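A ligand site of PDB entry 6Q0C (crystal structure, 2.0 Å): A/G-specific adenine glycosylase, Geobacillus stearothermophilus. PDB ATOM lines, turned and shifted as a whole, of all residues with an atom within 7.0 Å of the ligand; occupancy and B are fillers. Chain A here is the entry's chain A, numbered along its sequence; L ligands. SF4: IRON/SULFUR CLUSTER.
SG of Cys 208 lies close to N of Gln 211 (3.6 Å).
SG of Cys 208 lies close to N of Val 210.
O of Cys 205 sits close to OE1 of Gln 211 (3.5 Å).
SG of Cys 198 lies close to NH1 of Arg 153 (2.9 Å).
O of Arg 153 sits at hydrogen-bond distance from N of Ala 216, at 2.9 Å.
The guanidinium group of Arg 153 is in hydrogen-bond range of the backbone carbonyl oxygen of Thr 199 (2.8 Å).
The backbone carbonyl oxygen (O) of Pro 203 lies close to the side-chain sulfur (SG) of Cys 205, 3.7 Å away.
The backbone NH (N) of Cys 198 is in hydrogen-bond range of the backbone carbonyl oxygen (O) of Leu 193, 3.0 Å away.
SG of Cys 198 binds FE3 of the ligand, at 2.5 Å.
SG of Cys 205 binds FE2 of the ligand, 2.2 Å away.
The side-chain sulfur (SG) of Cys 208 is bound to an iron atom (FE1) of the ligand, at 2.4 Å.
The side-chain sulfur (SG) of Cys 214 binds an iron atom (FE4) of the ligand, 2.4 Å away.
A sulfur (S4) of the ligand sits close to the backbone NH (N) of Cys 205.
Residues that only touch the ligand: Arg 153 (3.7 Å), Leu 154 (3.6 Å), Val 197 (3.9 Å), Pro 203 (3.8 Å), Gln 211 (3.6 Å) and Ala 222 (3.8 Å).
Hydrophobic or aromatic side chains within 4 Å of the ligand: Leu 154, Val 197, Pro 203 and Ala 222.
Ten residues have an atom within 4 Å of the ligand: Arg 153, Leu 154, Val 197, Cys 198, Pro 203, Cys 205, Cys 208, Gln 211, Cys 214 and Ala 222.
The nearest printed residue that does not touch the ligand is Phe 217 (4.1 Å).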
ATOM      1  N   ARG A 149     -16.663 -18.803   4.185  1.00  0.00           N
ATOM      2  CA  ARG A 149     -16.129 -18.950   2.837  1.00  0.00           C
ATOM      3  C   ARG A 149     -14.706 -19.498   2.863  1.00  0.00           C
ATOM      4  O   ARG A 149     -14.378 -20.439   2.131  1.00  0.00           O
ATOM      5  CB  ARG A 149     -16.173 -17.614   2.102  1.00  0.00           C
ATOM      6  CG  ARG A 149     -15.358 -17.594   0.827  1.00  0.00           C
ATOM      7  CD  ARG A 149     -15.661 -16.367  -0.021  1.00  0.00           C
ATOM      8  NE  ARG A 149     -15.021 -15.172   0.518  1.00  0.00           N
ATOM      9  CZ  ARG A 149     -15.608 -14.302   1.334  1.00  0.00           C
ATOM     10  NH1 ARG A 149     -16.860 -14.469   1.727  1.00  0.00           N
ATOM     11  NH2 ARG A 149     -14.928 -13.250   1.761  1.00  0.00           N
ATOM     12  N   VAL A 150     -13.847 -18.922   3.706  1.00  0.00           N
ATOM     13  CA  VAL A 150     -12.466 -19.378   3.791  1.00  0.00           C
ATOM     14  C   VAL A 150     -12.418 -20.845   4.186  1.00  0.00           C
ATOM     15  O   VAL A 150     -11.808 -21.680   3.503  1.00  0.00           O
ATOM     16  CB  VAL A 150     -11.669 -18.505   4.775  1.00  0.00           C
ATOM     17  CG1 VAL A 150     -10.389 -19.207   5.196  1.00  0.00           C
ATOM     18  CG2 VAL A 150     -11.351 -17.154   4.160  1.00  0.00           C
ATOM     19  N   LEU A 151     -13.058 -21.192   5.316  1.00  0.00           N
ATOM     20  CA  LEU A 151     -13.012 -22.559   5.794  1.00  0.00           C
ATOM     21  C   LEU A 151     -13.639 -23.526   4.791  1.00  0.00           C
ATOM     22  O   LEU A 151     -13.132 -24.632   4.595  1.00  0.00           O
ATOM     23  CB  LEU A 151     -13.713 -22.661   7.151  1.00  0.00           C
ATOM     24  CG  LEU A 151     -13.083 -21.908   8.315  1.00  0.00           C
ATOM     25  CD1 LEU A 151     -13.850 -22.185   9.597  1.00  0.00           C
ATOM     26  CD2 LEU A 151     -11.617 -22.259   8.480  1.00  0.00           C
ATOM     27  N   ARG A 153     -13.539 -23.432   1.679  1.00  0.00           N
ATOM     28  CA  ARG A 153     -12.538 -23.722   0.664  1.00  0.00           C
ATOM     29  C   ARG A 153     -11.342 -24.456   1.251  1.00  0.00           C
ATOM     30  O   ARG A 153     -10.833 -25.416   0.645  1.00  0.00           O
ATOM     31  CB  ARG A 153     -12.073 -22.427   0.007  1.00  0.00           C
ATOM     32  CG  ARG A 153     -13.122 -21.786  -0.865  1.00  0.00           C
ATOM     33  CD  ARG A 153     -12.815 -20.315  -1.100  1.00  0.00           C
ATOM     34  NE  ARG A 153     -13.713 -19.726  -2.084  1.00  0.00           N
ATOM     35  CZ  ARG A 153     -13.702 -18.452  -2.436  1.00  0.00           C
ATOM     36  NH1 ARG A 153     -12.832 -17.616  -1.891  1.00  0.00           N
ATOM     37  NH2 ARG A 153     -14.567 -18.008  -3.338  1.00  0.00           N
ATOM     38  N   LEU A 154     -10.867 -24.016   2.426  1.00  0.00           N
ATOM     39  CA  LEU A 154      -9.723 -24.655   3.046  1.00  0.00           C
ATOM     40  C   LEU A 154      -9.951 -26.148   3.224  1.00  0.00           C
ATOM     41  O   LEU A 154      -9.102 -26.952   2.820  1.00  0.00           O
ATOM     42  CB  LEU A 154      -9.410 -24.009   4.397  1.00  0.00           C
ATOM     43  CG  LEU A 154      -8.587 -22.729   4.400  1.00  0.00           C
ATOM     44  CD1 LEU A 154      -8.074 -22.453   5.806  1.00  0.00           C
ATOM     45  CD2 LEU A 154      -7.428 -22.806   3.429  1.00  0.00           C
ATOM     46  N   LEU A 193      -8.292 -12.349   6.084  1.00  0.00           N
ATOM     47  CA  LEU A 193      -7.979 -13.201   4.949  1.00  0.00           C
ATOM     48  C   LEU A 193      -9.140 -13.230   3.954  1.00  0.00           C
ATOM     49  O   LEU A 193      -8.973 -12.910   2.776  1.00  0.00           O
ATOM     50  CB  LEU A 193      -7.649 -14.614   5.432  1.00  0.00           C
ATOM     51  CG  LEU A 193      -7.212 -15.591   4.346  1.00  0.00           C
ATOM     52  CD1 LEU A 193      -5.895 -15.158   3.727  1.00  0.00           C
ATOM     53  CD2 LEU A 193      -7.108 -17.004   4.902  1.00  0.00           C
ATOM     54  N   VAL A 197      -7.949 -11.520   0.609  1.00  0.00           N
ATOM     55  CA  VAL A 197      -7.356 -12.486  -0.314  1.00  0.00           C
ATOM     56  C   VAL A 197      -8.422 -13.458  -0.823  1.00  0.00           C
ATOM     57  O   VAL A 197      -8.766 -13.451  -2.004  1.00  0.00           O
ATOM     58  CB  VAL A 197      -6.202 -13.236   0.356  1.00  0.00           C
ATOM     59  CG1 VAL A 197      -5.658 -14.319  -0.556  1.00  0.00           C
ATOM     60  CG2 VAL A 197      -5.099 -12.268   0.759  1.00  0.00           C
ATOM     61  N   CYS A 198      -8.929 -14.312   0.072  1.00  0.00           N
ATOM     62  CA  CYS A 198      -9.903 -15.333  -0.297  1.00  0.00           C
ATOM     63  C   CYS A 198     -11.281 -14.675  -0.455  1.00  0.00           C
ATOM     64  O   CYS A 198     -12.189 -14.843   0.361  1.00  0.00           O
ATOM     65  CB  CYS A 198      -9.932 -16.450   0.734  1.00  0.00           C
ATOM     66  SG  CYS A 198     -10.981 -17.847   0.306  1.00  0.00           S
ATOM     67  N   THR A 199     -11.420 -13.931  -1.547  1.00  0.00           N
ATOM     68  CA  THR A 199     -12.596 -13.122  -1.772  1.00  0.00           C
ATOM     69  C   THR A 199     -13.738 -13.943  -2.361  1.00  0.00           C
ATOM     70  O   THR A 199     -13.536 -15.051  -2.859  1.00  0.00           O
ATOM     71  CB  THR A 199     -12.258 -11.968  -2.713  1.00  0.00           C
ATOM     72  OG1 THR A 199     -11.586 -12.474  -3.873  1.00  0.00           O
ATOM     73  CG2 THR A 199     -11.370 -10.948  -2.012  1.00  0.00           C
ATOM     74  N   PRO A 203     -10.621 -15.323  -5.940  1.00  0.00           N
ATOM     75  CA  PRO A 203      -9.682 -15.326  -4.809  1.00  0.00           C
ATOM     76  C   PRO A 203      -8.249 -15.364  -5.308  1.00  0.00           C
ATOM     77  O   PRO A 203      -7.937 -16.031  -6.302  1.00  0.00           O
ATOM     78  CB  PRO A 203     -10.050 -16.586  -4.031  1.00  0.00           C
ATOM     79  CG  PRO A 203     -10.687 -17.476  -5.043  1.00  0.00           C
ATOM     80  CD  PRO A 203     -11.432 -16.559  -5.965  1.00  0.00           C
ATOM     81  N   SER A 204      -7.369 -14.639  -4.621  1.00  0.00           N
ATOM     82  CA  SER A 204      -5.959 -14.583  -4.991  1.00  0.00           C
ATOM     83  C   SER A 204      -5.181 -15.722  -4.333  1.00  0.00           C
ATOM     84  O   SER A 204      -4.262 -15.528  -3.550  1.00  0.00           O
ATOM     85  CB  SER A 204      -5.373 -13.217  -4.630  1.00  0.00           C
ATOM     86  OG  SER A 204      -6.111 -12.178  -5.241  1.00  0.00           O
ATOM     87  N   CYS A 205      -5.607 -16.939  -4.684  1.00  0.00           N
ATOM     88  CA  CYS A 205      -4.990 -18.135  -4.108  1.00  0.00           C
ATOM     89  C   CYS A 205      -3.486 -18.137  -4.309  1.00  0.00           C
ATOM     90  O   CYS A 205      -2.732 -18.599  -3.435  1.00  0.00           O
ATOM     91  CB  CYS A 205      -5.617 -19.383  -4.743  1.00  0.00           C
ATOM     92  SG  CYS A 205      -7.428 -19.340  -4.822  1.00  0.00           S
ATOM     93  N   LEU A 206      -3.018 -17.623  -5.449  1.00  0.00           N
ATOM     94  CA  LEU A 206      -1.590 -17.582  -5.706  1.00  0.00           C
ATOM     95  C   LEU A 206      -0.855 -16.769  -4.651  1.00  0.00           C
ATOM     96  O   LEU A 206       0.270 -17.103  -4.266  1.00  0.00           O
ATOM     97  CB  LEU A 206      -1.325 -17.002  -7.102  1.00  0.00           C
ATOM     98  CG  LEU A 206      -1.799 -17.861  -8.280  1.00  0.00           C
ATOM     99  CD1 LEU A 206      -1.597 -17.139  -9.602  1.00  0.00           C
ATOM    100  CD2 LEU A 206      -1.085 -19.198  -8.291  1.00  0.00           C
ATOM    101  N   LEU A 207      -1.470 -15.687  -4.171  1.00  0.00           N
ATOM    102  CA  LEU A 207      -0.877 -14.860  -3.120  1.00  0.00           C
ATOM    103  C   LEU A 207      -1.240 -15.328  -1.716  1.00  0.00           C
ATOM    104  O   LEU A 207      -0.597 -14.897  -0.754  1.00  0.00           O
ATOM    105  CB  LEU A 207      -1.309 -13.404  -3.297  1.00  0.00           C
ATOM    106  CG  LEU A 207      -0.843 -12.703  -4.572  1.00  0.00           C
ATOM    107  CD1 LEU A 207      -1.481 -11.324  -4.677  1.00  0.00           C
ATOM    108  CD2 LEU A 207       0.677 -12.598  -4.611  1.00  0.00           C
ATOM    109  N   CYS A 208      -2.234 -16.204  -1.582  1.00  0.00           N
ATOM    110  CA  CYS A 208      -2.719 -16.579  -0.256  1.00  0.00           C
ATOM    111  C   CYS A 208      -1.583 -17.198   0.569  1.00  0.00           C
ATOM    112  O   CYS A 208      -0.811 -18.010   0.056  1.00  0.00           O
ATOM    113  CB  CYS A 208      -3.872 -17.577  -0.375  1.00  0.00           C
ATOM    114  SG  CYS A 208      -4.376 -18.326   1.184  1.00  0.00           S
ATOM    115  N   PRO A 209      -1.463 -16.830   1.851  1.00  0.00           N
ATOM    116  CA  PRO A 209      -0.422 -17.438   2.692  1.00  0.00           C
ATOM    117  C   PRO A 209      -0.685 -18.880   3.066  1.00  0.00           C
ATOM    118  O   PRO A 209       0.265 -19.599   3.384  1.00  0.00           O
ATOM    119  CB  PRO A 209      -0.414 -16.540   3.936  1.00  0.00           C
ATOM    120  CG  PRO A 209      -1.830 -16.107   4.031  1.00  0.00           C
ATOM    121  CD  PRO A 209      -2.230 -15.835   2.609  1.00  0.00           C
ATOM    122  N   VAL A 210      -1.947 -19.329   3.072  1.00  0.00           N
ATOM    123  CA  VAL A 210      -2.263 -20.688   3.487  1.00  0.00           C
ATOM    124  C   VAL A 210      -2.721 -21.522   2.298  1.00  0.00           C
ATOM    125  O   VAL A 210      -3.499 -22.468   2.452  1.00  0.00           O
ATOM    126  CB  VAL A 210      -3.312 -20.696   4.610  1.00  0.00           C
ATOM    127  CG1 VAL A 210      -2.713 -20.070   5.861  1.00  0.00           C
ATOM    128  CG2 VAL A 210      -4.584 -19.949   4.201  1.00  0.00           C
ATOM    129  N   GLN A 211      -2.221 -21.187   1.098  1.00  0.00           N
ATOM    130  CA  GLN A 211      -2.529 -21.978  -0.083  1.00  0.00           C
ATOM    131  C   GLN A 211      -2.141 -23.441   0.102  1.00  0.00           C
ATOM    132  O   GLN A 211      -2.878 -24.344  -0.298  1.00  0.00           O
ATOM    133  CB  GLN A 211      -1.816 -21.410  -1.312  1.00  0.00           C
ATOM    134  CG  GLN A 211      -2.044 -22.189  -2.592  1.00  0.00           C
ATOM    135  CD  GLN A 211      -0.928 -21.988  -3.593  1.00  0.00           C
ATOM    136  OE1 GLN A 211      -1.119 -21.404  -4.664  1.00  0.00           O
ATOM    137  NE2 GLN A 211       0.254 -22.493  -3.245  1.00  0.00           N
ATOM    138  N   ALA A 212      -0.962 -23.677   0.671  1.00  0.00           N
ATOM    139  CA  ALA A 212      -0.473 -25.049   0.821  1.00  0.00           C
ATOM    140  C   ALA A 212      -1.500 -25.949   1.501  1.00  0.00           C
ATOM    141  O   ALA A 212      -1.691 -27.092   1.084  1.00  0.00           O
ATOM    142  CB  ALA A 212       0.848 -25.037   1.606  1.00  0.00           C
ATOM    143  N   TYR A 213      -2.188 -25.438   2.530  1.00  0.00           N
ATOM    144  CA  TYR A 213      -3.138 -26.244   3.283  1.00  0.00           C
ATOM    145  C   TYR A 213      -4.545 -26.257   2.693  1.00  0.00           C
ATOM    146  O   TYR A 213      -5.429 -26.853   3.297  1.00  0.00           O
ATOM    147  CB  TYR A 213      -3.260 -25.738   4.732  1.00  0.00           C
ATOM    148  CG  TYR A 213      -1.984 -25.226   5.357  1.00  0.00           C
ATOM    149  CD1 TYR A 213      -1.557 -23.935   5.143  1.00  0.00           C
ATOM    150  CD2 TYR A 213      -1.246 -26.024   6.215  1.00  0.00           C
ATOM    151  CE1 TYR A 213      -0.411 -23.457   5.722  1.00  0.00           C
ATOM    152  CE2 TYR A 213      -0.080 -25.553   6.801  1.00  0.00           C
ATOM    153  CZ  TYR A 213       0.324 -24.262   6.549  1.00  0.00           C
ATOM    154  OH  TYR A 213       1.465 -23.765   7.118  1.00  0.00           O
ATOM    155  N   CYS A 214      -4.772 -25.622   1.544  1.00  0.00           N
ATOM    156  CA  CYS A 214      -6.128 -25.420   1.040  1.00  0.00           C
ATOM    157  C   CYS A 214      -6.520 -26.562   0.105  1.00  0.00           C
ATOM    158  O   CYS A 214      -5.921 -26.723  -0.964  1.00  0.00           O
ATOM    159  CB  CYS A 214      -6.255 -24.080   0.337  1.00  0.00           C
ATOM    160  SG  CYS A 214      -7.902 -23.809  -0.357  1.00  0.00           S
ATOM    161  N   GLN A 215      -7.548 -27.319   0.490  1.00  0.00           N
ATOM    162  CA  GLN A 215      -7.999 -28.428  -0.333  1.00  0.00           C
ATOM    163  C   GLN A 215      -8.746 -27.963  -1.585  1.00  0.00           C
ATOM    164  O   GLN A 215      -8.676 -28.620  -2.628  1.00  0.00           O
ATOM    165  CB  GLN A 215      -8.861 -29.359   0.522  1.00  0.00           C
ATOM    166  CG  GLN A 215      -7.989 -30.229   1.424  1.00  0.00           C
ATOM    167  CD  GLN A 215      -8.570 -30.492   2.804  1.00  0.00           C
ATOM    168  OE1 GLN A 215      -8.039 -30.019   3.808  1.00  0.00           O
ATOM    169  NE2 GLN A 215      -9.655 -31.251   2.851  1.00  0.00           N
ATOM    170  N   ALA A 216      -9.454 -26.831  -1.521  1.00  0.00           N
ATOM    171  CA  ALA A 216     -10.162 -26.342  -2.700  1.00  0.00           C
ATOM    172  C   ALA A 216      -9.194 -25.921  -3.804  1.00  0.00           C
ATOM    173  O   ALA A 216      -9.466 -26.129  -4.997  1.00  0.00           O
ATOM    174  CB  ALA A 216     -11.083 -25.180  -2.349  1.00  0.00           C
ATOM    175  N   PHE A 217      -8.056 -25.328  -3.436  1.00  0.00           N
ATOM    176  CA  PHE A 217      -7.082 -24.931  -4.446  1.00  0.00           C
ATOM    177  C   PHE A 217      -6.589 -26.140  -5.240  1.00  0.00           C
ATOM    178  O   PHE A 217      -6.525 -26.109  -6.471  1.00  0.00           O
ATOM    179  CB  PHE A 217      -5.895 -24.217  -3.805  1.00  0.00           C
ATOM    180  CG  PHE A 217      -4.832 -23.842  -4.792  1.00  0.00           C
ATOM    181  CD1 PHE A 217      -5.088 -22.912  -5.783  1.00  0.00           C
ATOM    182  CD2 PHE A 217      -3.578 -24.436  -4.753  1.00  0.00           C
ATOM    183  CE1 PHE A 217      -4.115 -22.563  -6.699  1.00  0.00           C
ATOM    184  CE2 PHE A 217      -2.599 -24.094  -5.665  1.00  0.00           C
ATOM    185  CZ  PHE A 217      -2.871 -23.153  -6.640  1.00  0.00           C
ATOM    186  N   VAL A 221     -11.475 -25.662  -7.468  1.00  0.00           N
ATOM    187  CA  VAL A 221     -12.896 -25.387  -7.278  1.00  0.00           C
ATOM    188  C   VAL A 221     -13.113 -24.208  -6.328  1.00  0.00           C
ATOM    189  O   VAL A 221     -14.188 -24.056  -5.763  1.00  0.00           O
ATOM    190  CB  VAL A 221     -13.636 -26.640  -6.782  1.00  0.00           C
ATOM    191  CG1 VAL A 221     -13.626 -27.717  -7.859  1.00  0.00           C
ATOM    192  CG2 VAL A 221     -13.018 -27.159  -5.495  1.00  0.00           C
ATOM    193  N   ALA A 222     -12.090 -23.368  -6.141  1.00  0.00           N
ATOM    194  CA  ALA A 222     -12.210 -22.228  -5.227  1.00  0.00           C
ATOM    195  C   ALA A 222     -13.425 -21.375  -5.560  1.00  0.00           C
ATOM    196  O   ALA A 222     -14.232 -21.051  -4.686  1.00  0.00           O
ATOM    197  CB  ALA A 222     -10.936 -21.396  -5.278  1.00  0.00           C
ATOM    198  N   GLU A 223     -13.579 -21.014  -6.837  1.00  0.00           N
ATOM    199  CA  GLU A 223     -14.676 -20.137  -7.237  1.00  0.00           C
ATOM    200  C   GLU A 223     -16.031 -20.734  -6.877  1.00  0.00           C
ATOM    201  O   GLU A 223     -16.950 -20.001  -6.501  1.00  0.00           O
ATOM    202  CB  GLU A 223     -14.592 -19.862  -8.733  1.00  0.00           C
ATOM    203  CG  GLU A 223     -13.766 -18.639  -9.099  1.00  0.00           C
ATOM    204  CD  GLU A 223     -13.318 -18.631 -10.552  1.00  0.00           C
ATOM    205  OE1 GLU A 223     -13.236 -19.725 -11.154  1.00  0.00           O
ATOM    206  OE2 GLU A 223     -13.050 -17.536 -11.083  1.00  0.00           O
HETATM  207 FE1  SF4 L   1      -6.207 -19.082  -0.183  1.00  0.00          FE
HETATM  208 FE2  SF4 L   1      -7.315 -19.688  -2.609  1.00  0.00          FE
HETATM  209 FE3  SF4 L   1      -8.929 -19.055  -0.488  1.00  0.00          FE
HETATM  210 FE4  SF4 L   1      -7.581 -21.428  -0.520  1.00  0.00          FE
HETATM  211  S1  SF4 L   1      -9.210 -20.769  -1.958  1.00  0.00           S
HETATM  212  S2  SF4 L   1      -7.759 -19.971   1.233  1.00  0.00           S
HETATM  213  S3  SF4 L   1      -5.638 -20.816  -1.553  1.00  0.00           S
HETATM  214  S4  SF4 L   1      -7.423 -17.684  -1.529  1.00  0.00           S
